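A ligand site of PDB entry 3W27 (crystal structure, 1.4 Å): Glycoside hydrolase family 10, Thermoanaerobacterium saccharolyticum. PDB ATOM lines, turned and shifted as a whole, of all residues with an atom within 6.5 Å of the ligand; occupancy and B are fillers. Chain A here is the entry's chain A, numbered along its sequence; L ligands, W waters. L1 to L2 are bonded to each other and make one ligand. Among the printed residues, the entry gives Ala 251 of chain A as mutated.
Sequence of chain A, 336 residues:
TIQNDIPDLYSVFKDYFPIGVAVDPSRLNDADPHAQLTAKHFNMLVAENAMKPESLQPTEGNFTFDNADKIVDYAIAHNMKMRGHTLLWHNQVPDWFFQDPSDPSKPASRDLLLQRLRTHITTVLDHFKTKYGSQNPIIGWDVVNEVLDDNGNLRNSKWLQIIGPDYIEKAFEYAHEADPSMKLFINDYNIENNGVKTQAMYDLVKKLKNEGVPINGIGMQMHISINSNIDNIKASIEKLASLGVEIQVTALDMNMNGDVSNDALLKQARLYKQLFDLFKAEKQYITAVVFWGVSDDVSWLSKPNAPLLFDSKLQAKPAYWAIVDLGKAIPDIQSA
O1 of LG2 L2 lies within hydrogen-bond range of OE2 of Glu 48 (2.7 Å).
NE2 of His 223 lies within hydrogen-bond range of O1 of LIG L1 (2.7 Å).
A ring nitrogen (NE2) of His 85 lies within hydrogen-bond range of an oxygen (O3) of LIG L1 (2.8 Å).
NE1 of Trp 292 is in hydrogen-bond range of O1 of LG2 L2 (2.8 Å).
An oxygen (O3) of LIG L1 lies within hydrogen-bond range of the side-chain amino group of Lys 52 (2.9 Å).
The side-chain amide nitrogen of Asn 145 is in hydrogen-bond range of an oxygen (O2) of LIG L1 (2.9 Å).
The side-chain amide nitrogen (ND2) of Asn 49 sits at hydrogen-bond distance from an oxygen (O2) of LG2 L2, at 3.0 Å.
The side-chain amide oxygen of Gln 92 lies close to an oxygen (O4) of LG2 L2, 3.2 Å away.
The side-chain amide oxygen (OE1) of Gln 221 sits at hydrogen-bond distance from an oxygen (O2) of LIG L1 (3.2 Å).
Water W5 bridges an oxygen (O5) of LIG L1 (2.7 Å) and the side-chain carboxylate of Glu 146 (3.0 Å).
Water W4 lies within hydrogen-bond range of the side-chain amide nitrogen of Gln 221, an oxygen (O5) of LIG L1 and the side-chain carboxylate of Glu 146.
ND1 of His 85 sits at hydrogen-bond distance from OD2 of Asp 142.
The side-chain amide oxygen of Asn 49 lies within hydrogen-bond range of the side-chain amino group of Lys 52 (2.8 Å).
The side-chain amide oxygen (OE1) of Gln 92 sits at hydrogen-bond distance from the side-chain amino group (NZ) of Lys 52, at 2.9 Å.
OD1 of Asn 145 lies close to OE1 of Gln 221, 3.4 Å away.
NE1 of Trp 89 sits close to ND2 of Asn 145.
The side-chain amide nitrogen of Asn 187 is in hydrogen-bond range of the side-chain amide oxygen of Asn 145, 2.9 Å away.
The side-chain amide oxygen (OE1) of Gln 221 lies close to the side-chain amide nitrogen (ND2) of Asn 187, at 3.5 Å.
The indole nitrogen (NE1) of Trp 89 lies within hydrogen-bond range of the side-chain carboxylate (OE1) of Glu 146 (2.8 Å).
Residues that only touch the ligand: Trp 300, Trp 89, Ala 251 and Glu 146.
Hydrophobic or aromatic side chains that line the ligand: His 85, Trp 89, His 223, Ala 251, Trp 292 and Trp 300.
Within 4 Å of the ligand: Glu 48, Asn 49, Lys 52, His 85, Trp 89, Gln 92, Asn 145, Glu 146, Gln 221, His 223, Ala 251, Trp 292 and Trp 300.
Along chain A the residues within 4 Å of the ligand span positions 48 to 300.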
ATOM      1  N   GLU A  48     -24.607 -16.990   2.635  1.00  0.00           N
ATOM      2  CA  GLU A  48     -23.230 -16.702   2.245  1.00  0.00           C
ATOM      3  C   GLU A  48     -22.238 -17.215   3.298  1.00  0.00           C
ATOM      4  O   GLU A  48     -21.149 -17.681   2.935  1.00  0.00           O
ATOM      5  CB  GLU A  48     -23.065 -15.182   2.052  1.00  0.00           C
ATOM      6  CG  GLU A  48     -21.720 -14.785   1.451  1.00  0.00           C
ATOM      7  CD  GLU A  48     -21.557 -13.306   1.250  1.00  0.00           C
ATOM      8  OE1 GLU A  48     -22.402 -12.514   1.727  1.00  0.00           O
ATOM      9  OE2 GLU A  48     -20.549 -12.919   0.614  1.00  0.00           O
ATOM     10  N   ASN A  49     -22.634 -17.138   4.558  1.00  0.00           N
ATOM     11  CA  ASN A  49     -21.766 -17.564   5.676  1.00  0.00           C
ATOM     12  C   ASN A  49     -22.474 -18.271   6.827  1.00  0.00           C
ATOM     13  O   ASN A  49     -21.855 -19.066   7.516  1.00  0.00           O
ATOM     14  CB  ASN A  49     -21.074 -16.356   6.275  1.00  0.00           C
ATOM     15  CG  ASN A  49     -20.033 -15.779   5.337  1.00  0.00           C
ATOM     16  OD1 ASN A  49     -19.038 -16.454   5.017  1.00  0.00           O
ATOM     17  ND2 ASN A  49     -20.243 -14.549   4.862  1.00  0.00           N
ATOM     18  N   LYS A  52     -22.039 -22.218   7.477  1.00  0.00           N
ATOM     19  CA  LYS A  52     -20.705 -22.793   7.490  1.00  0.00           C
ATOM     20  C   LYS A  52     -20.420 -23.408   8.872  1.00  0.00           C
ATOM     21  O   LYS A  52     -21.047 -23.051   9.861  1.00  0.00           O
ATOM     22  CB  LYS A  52     -19.657 -21.730   7.138  1.00  0.00           C
ATOM     23  CG  LYS A  52     -19.721 -21.397   5.636  1.00  0.00           C
ATOM     24  CD  LYS A  52     -18.890 -20.186   5.281  1.00  0.00           C
ATOM     25  CE  LYS A  52     -18.997 -19.912   3.768  1.00  0.00           C
ATOM     26  NZ  LYS A  52     -18.328 -18.628   3.364  1.00  0.00           N
ATOM     27  N   HIS A  85     -25.079 -24.475   2.422  1.00  0.00           N
ATOM     28  CA  HIS A  85     -23.646 -24.294   2.215  1.00  0.00           C
ATOM     29  C   HIS A  85     -23.028 -24.018   3.588  1.00  0.00           C
ATOM     30  O   HIS A  85     -23.346 -22.996   4.200  1.00  0.00           O
ATOM     31  CB  HIS A  85     -23.427 -23.086   1.284  1.00  0.00           C
ATOM     32  CG  HIS A  85     -21.985 -22.802   1.007  1.00  0.00           C
ATOM     33  ND1 HIS A  85     -21.247 -23.558   0.135  1.00  0.00           N
ATOM     34  CD2 HIS A  85     -21.146 -21.856   1.503  1.00  0.00           C
ATOM     35  CE1 HIS A  85     -20.008 -23.083   0.089  1.00  0.00           C
ATOM     36  NE2 HIS A  85     -19.923 -22.060   0.916  1.00  0.00           N
ATOM     37  N   THR A  86     -22.147 -24.875   4.130  1.00  0.00           N
ATOM     38  CA  THR A  86     -21.643 -26.127   3.578  1.00  0.00           C
ATOM     39  C   THR A  86     -21.275 -26.983   4.816  1.00  0.00           C
ATOM     40  O   THR A  86     -20.892 -26.447   5.860  1.00  0.00           O
ATOM     41  CB  THR A  86     -20.377 -25.892   2.693  1.00  0.00           C
ATOM     42  OG1 THR A  86     -19.816 -27.140   2.276  1.00  0.00           O
ATOM     43  CG2 THR A  86     -19.306 -25.087   3.447  1.00  0.00           C
ATOM     44  N   TRP A  89     -15.492 -27.939   5.105  1.00  0.00           N
ATOM     45  CA  TRP A  89     -14.615 -27.055   4.349  1.00  0.00           C
ATOM     46  C   TRP A  89     -13.346 -26.926   5.206  1.00  0.00           C
ATOM     47  O   TRP A  89     -13.362 -27.309   6.399  1.00  0.00           O
ATOM     48  CB  TRP A  89     -15.313 -25.696   4.169  1.00  0.00           C
ATOM     49  CG  TRP A  89     -14.649 -24.769   3.180  1.00  0.00           C
ATOM     50  CD1 TRP A  89     -13.806 -25.102   2.149  1.00  0.00           C
ATOM     51  CD2 TRP A  89     -14.864 -23.359   3.086  1.00  0.00           C
ATOM     52  NE1 TRP A  89     -13.480 -23.972   1.408  1.00  0.00           N
ATOM     53  CE2 TRP A  89     -14.114 -22.896   1.958  1.00  0.00           C
ATOM     54  CE3 TRP A  89     -15.611 -22.443   3.833  1.00  0.00           C
ATOM     55  CZ2 TRP A  89     -14.105 -21.552   1.564  1.00  0.00           C
ATOM     56  CZ3 TRP A  89     -15.591 -21.115   3.440  1.00  0.00           C
ATOM     57  CH2 TRP A  89     -14.849 -20.671   2.320  1.00  0.00           C
ATOM     58  N   GLN A  92     -13.255 -21.408   7.566  1.00  0.00           N
ATOM     59  CA  GLN A  92     -14.433 -21.125   8.389  1.00  0.00           C
ATOM     60  C   GLN A  92     -14.955 -22.358   9.104  1.00  0.00           C
ATOM     61  O   GLN A  92     -16.156 -22.651   9.166  1.00  0.00           O
ATOM     62  CB  GLN A  92     -15.499 -20.441   7.501  1.00  0.00           C
ATOM     63  CG  GLN A  92     -15.124 -18.967   7.235  1.00  0.00           C
ATOM     64  CD  GLN A  92     -16.111 -18.297   6.349  1.00  0.00           C
ATOM     65  OE1 GLN A  92     -15.991 -18.344   5.121  1.00  0.00           O
ATOM     66  NE2 GLN A  92     -17.120 -17.647   6.956  1.00  0.00           N
ATOM     67  N   ASP A 142     -24.114 -28.672  -0.003  1.00  0.00           N
ATOM     68  CA  ASP A 142     -22.723 -28.797  -0.449  1.00  0.00           C
ATOM     69  C   ASP A 142     -22.165 -29.582   0.761  1.00  0.00           C
ATOM     70  O   ASP A 142     -21.903 -29.024   1.836  1.00  0.00           O
ATOM     71  CB  ASP A 142     -22.026 -27.441  -0.557  1.00  0.00           C
ATOM     72  CG  ASP A 142     -22.438 -26.669  -1.765  1.00  0.00           C
ATOM     73  OD1 ASP A 142     -22.694 -27.309  -2.815  1.00  0.00           O
ATOM     74  OD2 ASP A 142     -22.451 -25.425  -1.637  1.00  0.00           O
ATOM     75  N   ASN A 145     -16.737 -28.979   0.403  1.00  0.00           N
ATOM     76  CA  ASN A 145     -16.394 -27.788  -0.375  1.00  0.00           C
ATOM     77  C   ASN A 145     -14.893 -27.717  -0.557  1.00  0.00           C
ATOM     78  O   ASN A 145     -14.141 -27.852   0.415  1.00  0.00           O
ATOM     79  CB  ASN A 145     -16.866 -26.566   0.417  1.00  0.00           C
ATOM     80  CG  ASN A 145     -16.960 -25.289  -0.427  1.00  0.00           C
ATOM     81  OD1 ASN A 145     -17.382 -25.345  -1.594  1.00  0.00           O
ATOM     82  ND2 ASN A 145     -16.606 -24.143   0.143  1.00  0.00           N
ATOM     83  N   GLU A 146     -14.450 -27.501  -1.784  1.00  0.00           N
ATOM     84  CA  GLU A 146     -13.041 -27.296  -2.101  1.00  0.00           C
ATOM     85  C   GLU A 146     -12.071 -28.356  -1.621  1.00  0.00           C
ATOM     86  O   GLU A 146     -11.006 -28.054  -1.052  1.00  0.00           O
ATOM     87  CB  GLU A 146     -12.626 -25.917  -1.581  1.00  0.00           C
ATOM     88  CG  GLU A 146     -13.505 -24.800  -2.218  1.00  0.00           C
ATOM     89  CD  GLU A 146     -13.129 -23.394  -1.782  1.00  0.00           C
ATOM     90  OE1 GLU A 146     -12.177 -23.249  -0.985  1.00  0.00           O
ATOM     91  OE2 GLU A 146     -13.796 -22.427  -2.228  1.00  0.00           O
ATOM     92  N   ASN A 187     -18.665 -29.441  -4.110  1.00  0.00           N
ATOM     93  CA  ASN A 187     -18.556 -28.087  -4.703  1.00  0.00           C
ATOM     94  C   ASN A 187     -17.122 -27.622  -4.850  1.00  0.00           C
ATOM     95  O   ASN A 187     -16.275 -27.907  -3.979  1.00  0.00           O
ATOM     96  CB  ASN A 187     -19.311 -27.135  -3.747  1.00  0.00           C
ATOM     97  CG  ASN A 187     -19.629 -25.757  -4.346  1.00  0.00           C
ATOM     98  OD1 ASN A 187     -20.189 -25.649  -5.446  1.00  0.00           O
ATOM     99  ND2 ASN A 187     -19.314 -24.690  -3.606  1.00  0.00           N
ATOM    100  N   TYR A 189     -14.230 -24.598  -7.057  1.00  0.00           N
ATOM    101  CA  TYR A 189     -13.881 -23.518  -7.997  1.00  0.00           C
ATOM    102  C   TYR A 189     -12.825 -24.011  -8.977  1.00  0.00           C
ATOM    103  O   TYR A 189     -12.139 -25.004  -8.725  1.00  0.00           O
ATOM    104  CB  TYR A 189     -13.365 -22.256  -7.251  1.00  0.00           C
ATOM    105  CG  TYR A 189     -12.060 -22.413  -6.509  1.00  0.00           C
ATOM    106  CD1 TYR A 189     -10.838 -22.085  -7.105  1.00  0.00           C
ATOM    107  CD2 TYR A 189     -12.053 -22.907  -5.201  1.00  0.00           C
ATOM    108  CE1 TYR A 189      -9.643 -22.243  -6.417  1.00  0.00           C
ATOM    109  CE2 TYR A 189     -10.886 -23.073  -4.501  1.00  0.00           C
ATOM    110  CZ  TYR A 189      -9.683 -22.748  -5.111  1.00  0.00           C
ATOM    111  OH  TYR A 189      -8.500 -22.941  -4.419  1.00  0.00           O
ATOM    112  N   GLN A 221     -18.629 -23.607  -8.554  1.00  0.00           N
ATOM    113  CA  GLN A 221     -18.709 -22.242  -8.018  1.00  0.00           C
ATOM    114  C   GLN A 221     -18.837 -21.124  -9.086  1.00  0.00           C
ATOM    115  O   GLN A 221     -19.636 -20.184  -8.945  1.00  0.00           O
ATOM    116  CB  GLN A 221     -17.496 -21.973  -7.101  1.00  0.00           C
ATOM    117  CG  GLN A 221     -17.600 -22.691  -5.773  1.00  0.00           C
ATOM    118  CD  GLN A 221     -16.372 -22.490  -4.893  1.00  0.00           C
ATOM    119  OE1 GLN A 221     -16.162 -23.234  -3.895  1.00  0.00           O
ATOM    120  NE2 GLN A 221     -15.559 -21.520  -5.230  1.00  0.00           N
ATOM    121  N   HIS A 223     -16.557 -18.706 -10.128  1.00  0.00           N
ATOM    122  CA  HIS A 223     -16.011 -17.383  -9.839  1.00  0.00           C
ATOM    123  C   HIS A 223     -15.161 -17.119 -11.076  1.00  0.00           C
ATOM    124  O   HIS A 223     -13.956 -17.366 -11.107  1.00  0.00           O
ATOM    125  CB  HIS A 223     -15.149 -17.447  -8.573  1.00  0.00           C
ATOM    126  CG  HIS A 223     -15.955 -17.651  -7.325  1.00  0.00           C
ATOM    127  ND1 HIS A 223     -16.848 -16.719  -6.845  1.00  0.00           N
ATOM    128  CD2 HIS A 223     -16.004 -18.695  -6.456  1.00  0.00           C
ATOM    129  CE1 HIS A 223     -17.418 -17.170  -5.744  1.00  0.00           C
ATOM    130  NE2 HIS A 223     -16.930 -18.368  -5.485  1.00  0.00           N
ATOM    131  N   THR A 250     -23.072 -22.749  -8.505  1.00  0.00           N
ATOM    132  CA  THR A 250     -23.320 -22.346  -7.133  1.00  0.00           C
ATOM    133  C   THR A 250     -22.856 -21.002  -6.595  1.00  0.00           C
ATOM    134  O   THR A 250     -23.401 -20.569  -5.602  1.00  0.00           O
ATOM    135  CB  THR A 250     -22.756 -23.429  -6.212  1.00  0.00           C
ATOM    136  OG1 THR A 250     -21.339 -23.490  -6.424  1.00  0.00           O
ATOM    137  CG2 THR A 250     -23.329 -24.802  -6.543  1.00  0.00           C
ATOM    138  N   ALA A 251     -21.915 -20.326  -7.238  1.00  0.00           N
ATOM    139  CA  ALA A 251     -21.404 -19.058  -6.667  1.00  0.00           C
ATOM    140  C   ALA A 251     -20.906 -18.061  -7.715  1.00  0.00           C
ATOM    141  O   ALA A 251     -19.840 -17.413  -7.576  1.00  0.00           O
ATOM    142  CB  ALA A 251     -20.282 -19.362  -5.690  1.00  0.00           C
ATOM    143  N   TRP A 292     -23.174 -15.161  -6.284  1.00  0.00           N
ATOM    144  CA  TRP A 292     -22.563 -15.047  -4.965  1.00  0.00           C
ATOM    145  C   TRP A 292     -22.577 -13.620  -4.448  1.00  0.00           C
ATOM    146  O   TRP A 292     -21.564 -12.929  -4.372  1.00  0.00           O
ATOM    147  CB  TRP A 292     -21.154 -15.652  -4.955  1.00  0.00           C
ATOM    148  CG  TRP A 292     -20.756 -16.092  -3.577  1.00  0.00           C
ATOM    149  CD1 TRP A 292     -19.888 -15.463  -2.735  1.00  0.00           C
ATOM    150  CD2 TRP A 292     -21.317 -17.189  -2.850  1.00  0.00           C
ATOM    151  NE1 TRP A 292     -19.877 -16.101  -1.512  1.00  0.00           N
ATOM    152  CE2 TRP A 292     -20.750 -17.162  -1.555  1.00  0.00           C
ATOM    153  CE3 TRP A 292     -22.254 -18.183  -3.168  1.00  0.00           C
ATOM    154  CZ2 TRP A 292     -21.101 -18.098  -0.551  1.00  0.00           C
ATOM    155  CZ3 TRP A 292     -22.603 -19.120  -2.186  1.00  0.00           C
ATOM    156  CH2 TRP A 292     -22.034 -19.067  -0.901  1.00  0.00           C
ATOM    157  N   SER A 299     -20.417  -7.565  -2.565  1.00  0.00           N
ATOM    158  CA  SER A 299     -19.646  -8.696  -3.084  1.00  0.00           C
ATOM    159  C   SER A 299     -18.428  -8.947  -2.208  1.00  0.00           C
ATOM    160  O   SER A 299     -17.779  -8.011  -1.727  1.00  0.00           O
ATOM    161  CB  SER A 299     -19.149  -8.390  -4.489  1.00  0.00           C
ATOM    162  OG  SER A 299     -18.225  -9.385  -4.946  1.00  0.00           O
ATOM    163  N   TRP A 300     -18.078 -10.223  -2.057  1.00  0.00           N
ATOM    164  CA  TRP A 300     -16.916 -10.613  -1.272  1.00  0.00           C
ATOM    165  C   TRP A 300     -15.575 -10.278  -1.962  1.00  0.00           C
ATOM    166  O   TRP A 300     -14.524 -10.348  -1.323  1.00  0.00           O
ATOM    167  CB  TRP A 300     -16.930 -12.123  -0.987  1.00  0.00           C
ATOM    168  CG  TRP A 300     -16.664 -12.992  -2.180  1.00  0.00           C
ATOM    169  CD1 TRP A 300     -17.336 -13.016  -3.366  1.00  0.00           C
ATOM    170  CD2 TRP A 300     -15.624 -13.969  -2.274  1.00  0.00           C
ATOM    171  NE1 TRP A 300     -16.785 -13.951  -4.199  1.00  0.00           N
ATOM    172  CE2 TRP A 300     -15.734 -14.553  -3.552  1.00  0.00           C
ATOM    173  CE3 TRP A 300     -14.613 -14.406  -1.406  1.00  0.00           C
ATOM    174  CZ2 TRP A 300     -14.863 -15.549  -3.983  1.00  0.00           C
ATOM    175  CZ3 TRP A 300     -13.758 -15.389  -1.824  1.00  0.00           C
ATOM    176  CH2 TRP A 300     -13.883 -15.960  -3.112  1.00  0.00           C
HETATM  177  C1  LIG L   1     -16.503 -19.910  -2.532  1.00  0.00           C
HETATM  178  C2  LIG L   1     -16.829 -20.519  -1.170  1.00  0.00           C
HETATM  179  C3  LIG L   1     -17.668 -19.542  -0.360  1.00  0.00           C
HETATM  180  C4  LIG L   1     -16.893 -18.245  -0.231  1.00  0.00           C
HETATM  181  C5  LIG L   1     -16.626 -17.711  -1.628  1.00  0.00           C
HETATM  182  O1  LIG L   1     -17.697 -19.720  -3.297  1.00  0.00           O
HETATM  183  O2  LIG L   1     -17.517 -21.764  -1.342  1.00  0.00           O
HETATM  184  O3  LIG L   1     -17.914 -20.081   0.944  1.00  0.00           O
HETATM  185  O4  LIG L   1     -17.715 -17.313   0.500  1.00  0.00           O
HETATM  186  O5  LIG L   1     -15.817 -18.664  -2.337  1.00  0.00           O
HETATM  187  C1  LG2 L   2     -16.932 -16.298   1.134  1.00  0.00           C
HETATM  188  C2  LG2 L   2     -17.906 -15.248   1.644  1.00  0.00           C
HETATM  189  C3  LG2 L   2     -17.191 -14.205   2.487  1.00  0.00           C
HETATM  190  C4  LG2 L   2     -16.396 -14.906   3.574  1.00  0.00           C
HETATM  191  C5  LG2 L   2     -15.463 -15.922   2.934  1.00  0.00           C
HETATM  192  O1  LG2 L   2     -18.514 -14.623   0.501  1.00  0.00           O
HETATM  193  O2  LG2 L   2     -18.166 -13.361   3.119  1.00  0.00           O
HETATM  194  O3  LG2 L   2     -15.596 -13.924   4.268  1.00  0.00           O
HETATM  195  O4  LG2 L   2     -16.263 -16.904   2.240  1.00  0.00           O
HETATM  196  O   HOH W   1     -17.357 -12.549   6.101  1.00  0.00           O
HETATM  197  O   HOH W   2     -19.912 -21.102  -2.610  1.00  0.00           O
HETATM  198  O   HOH W   3     -14.230 -15.016   6.445  1.00  0.00           O
HETATM  199  O   HOH W   4     -13.487 -19.758  -4.438  1.00  0.00           O
HETATM  200  O   HOH W   5     -13.402 -19.541  -1.543  1.00  0.00           O
HETATM  201  O   HOH W   6     -13.663 -12.776   2.627  1.00  0.00           O
HETATM  202  O   HOH W   7     -13.293 -18.390   4.101  1.00  0.00           O
HETATM  203  O   HOH W   8     -17.472 -10.802   2.557  1.00  0.00           O
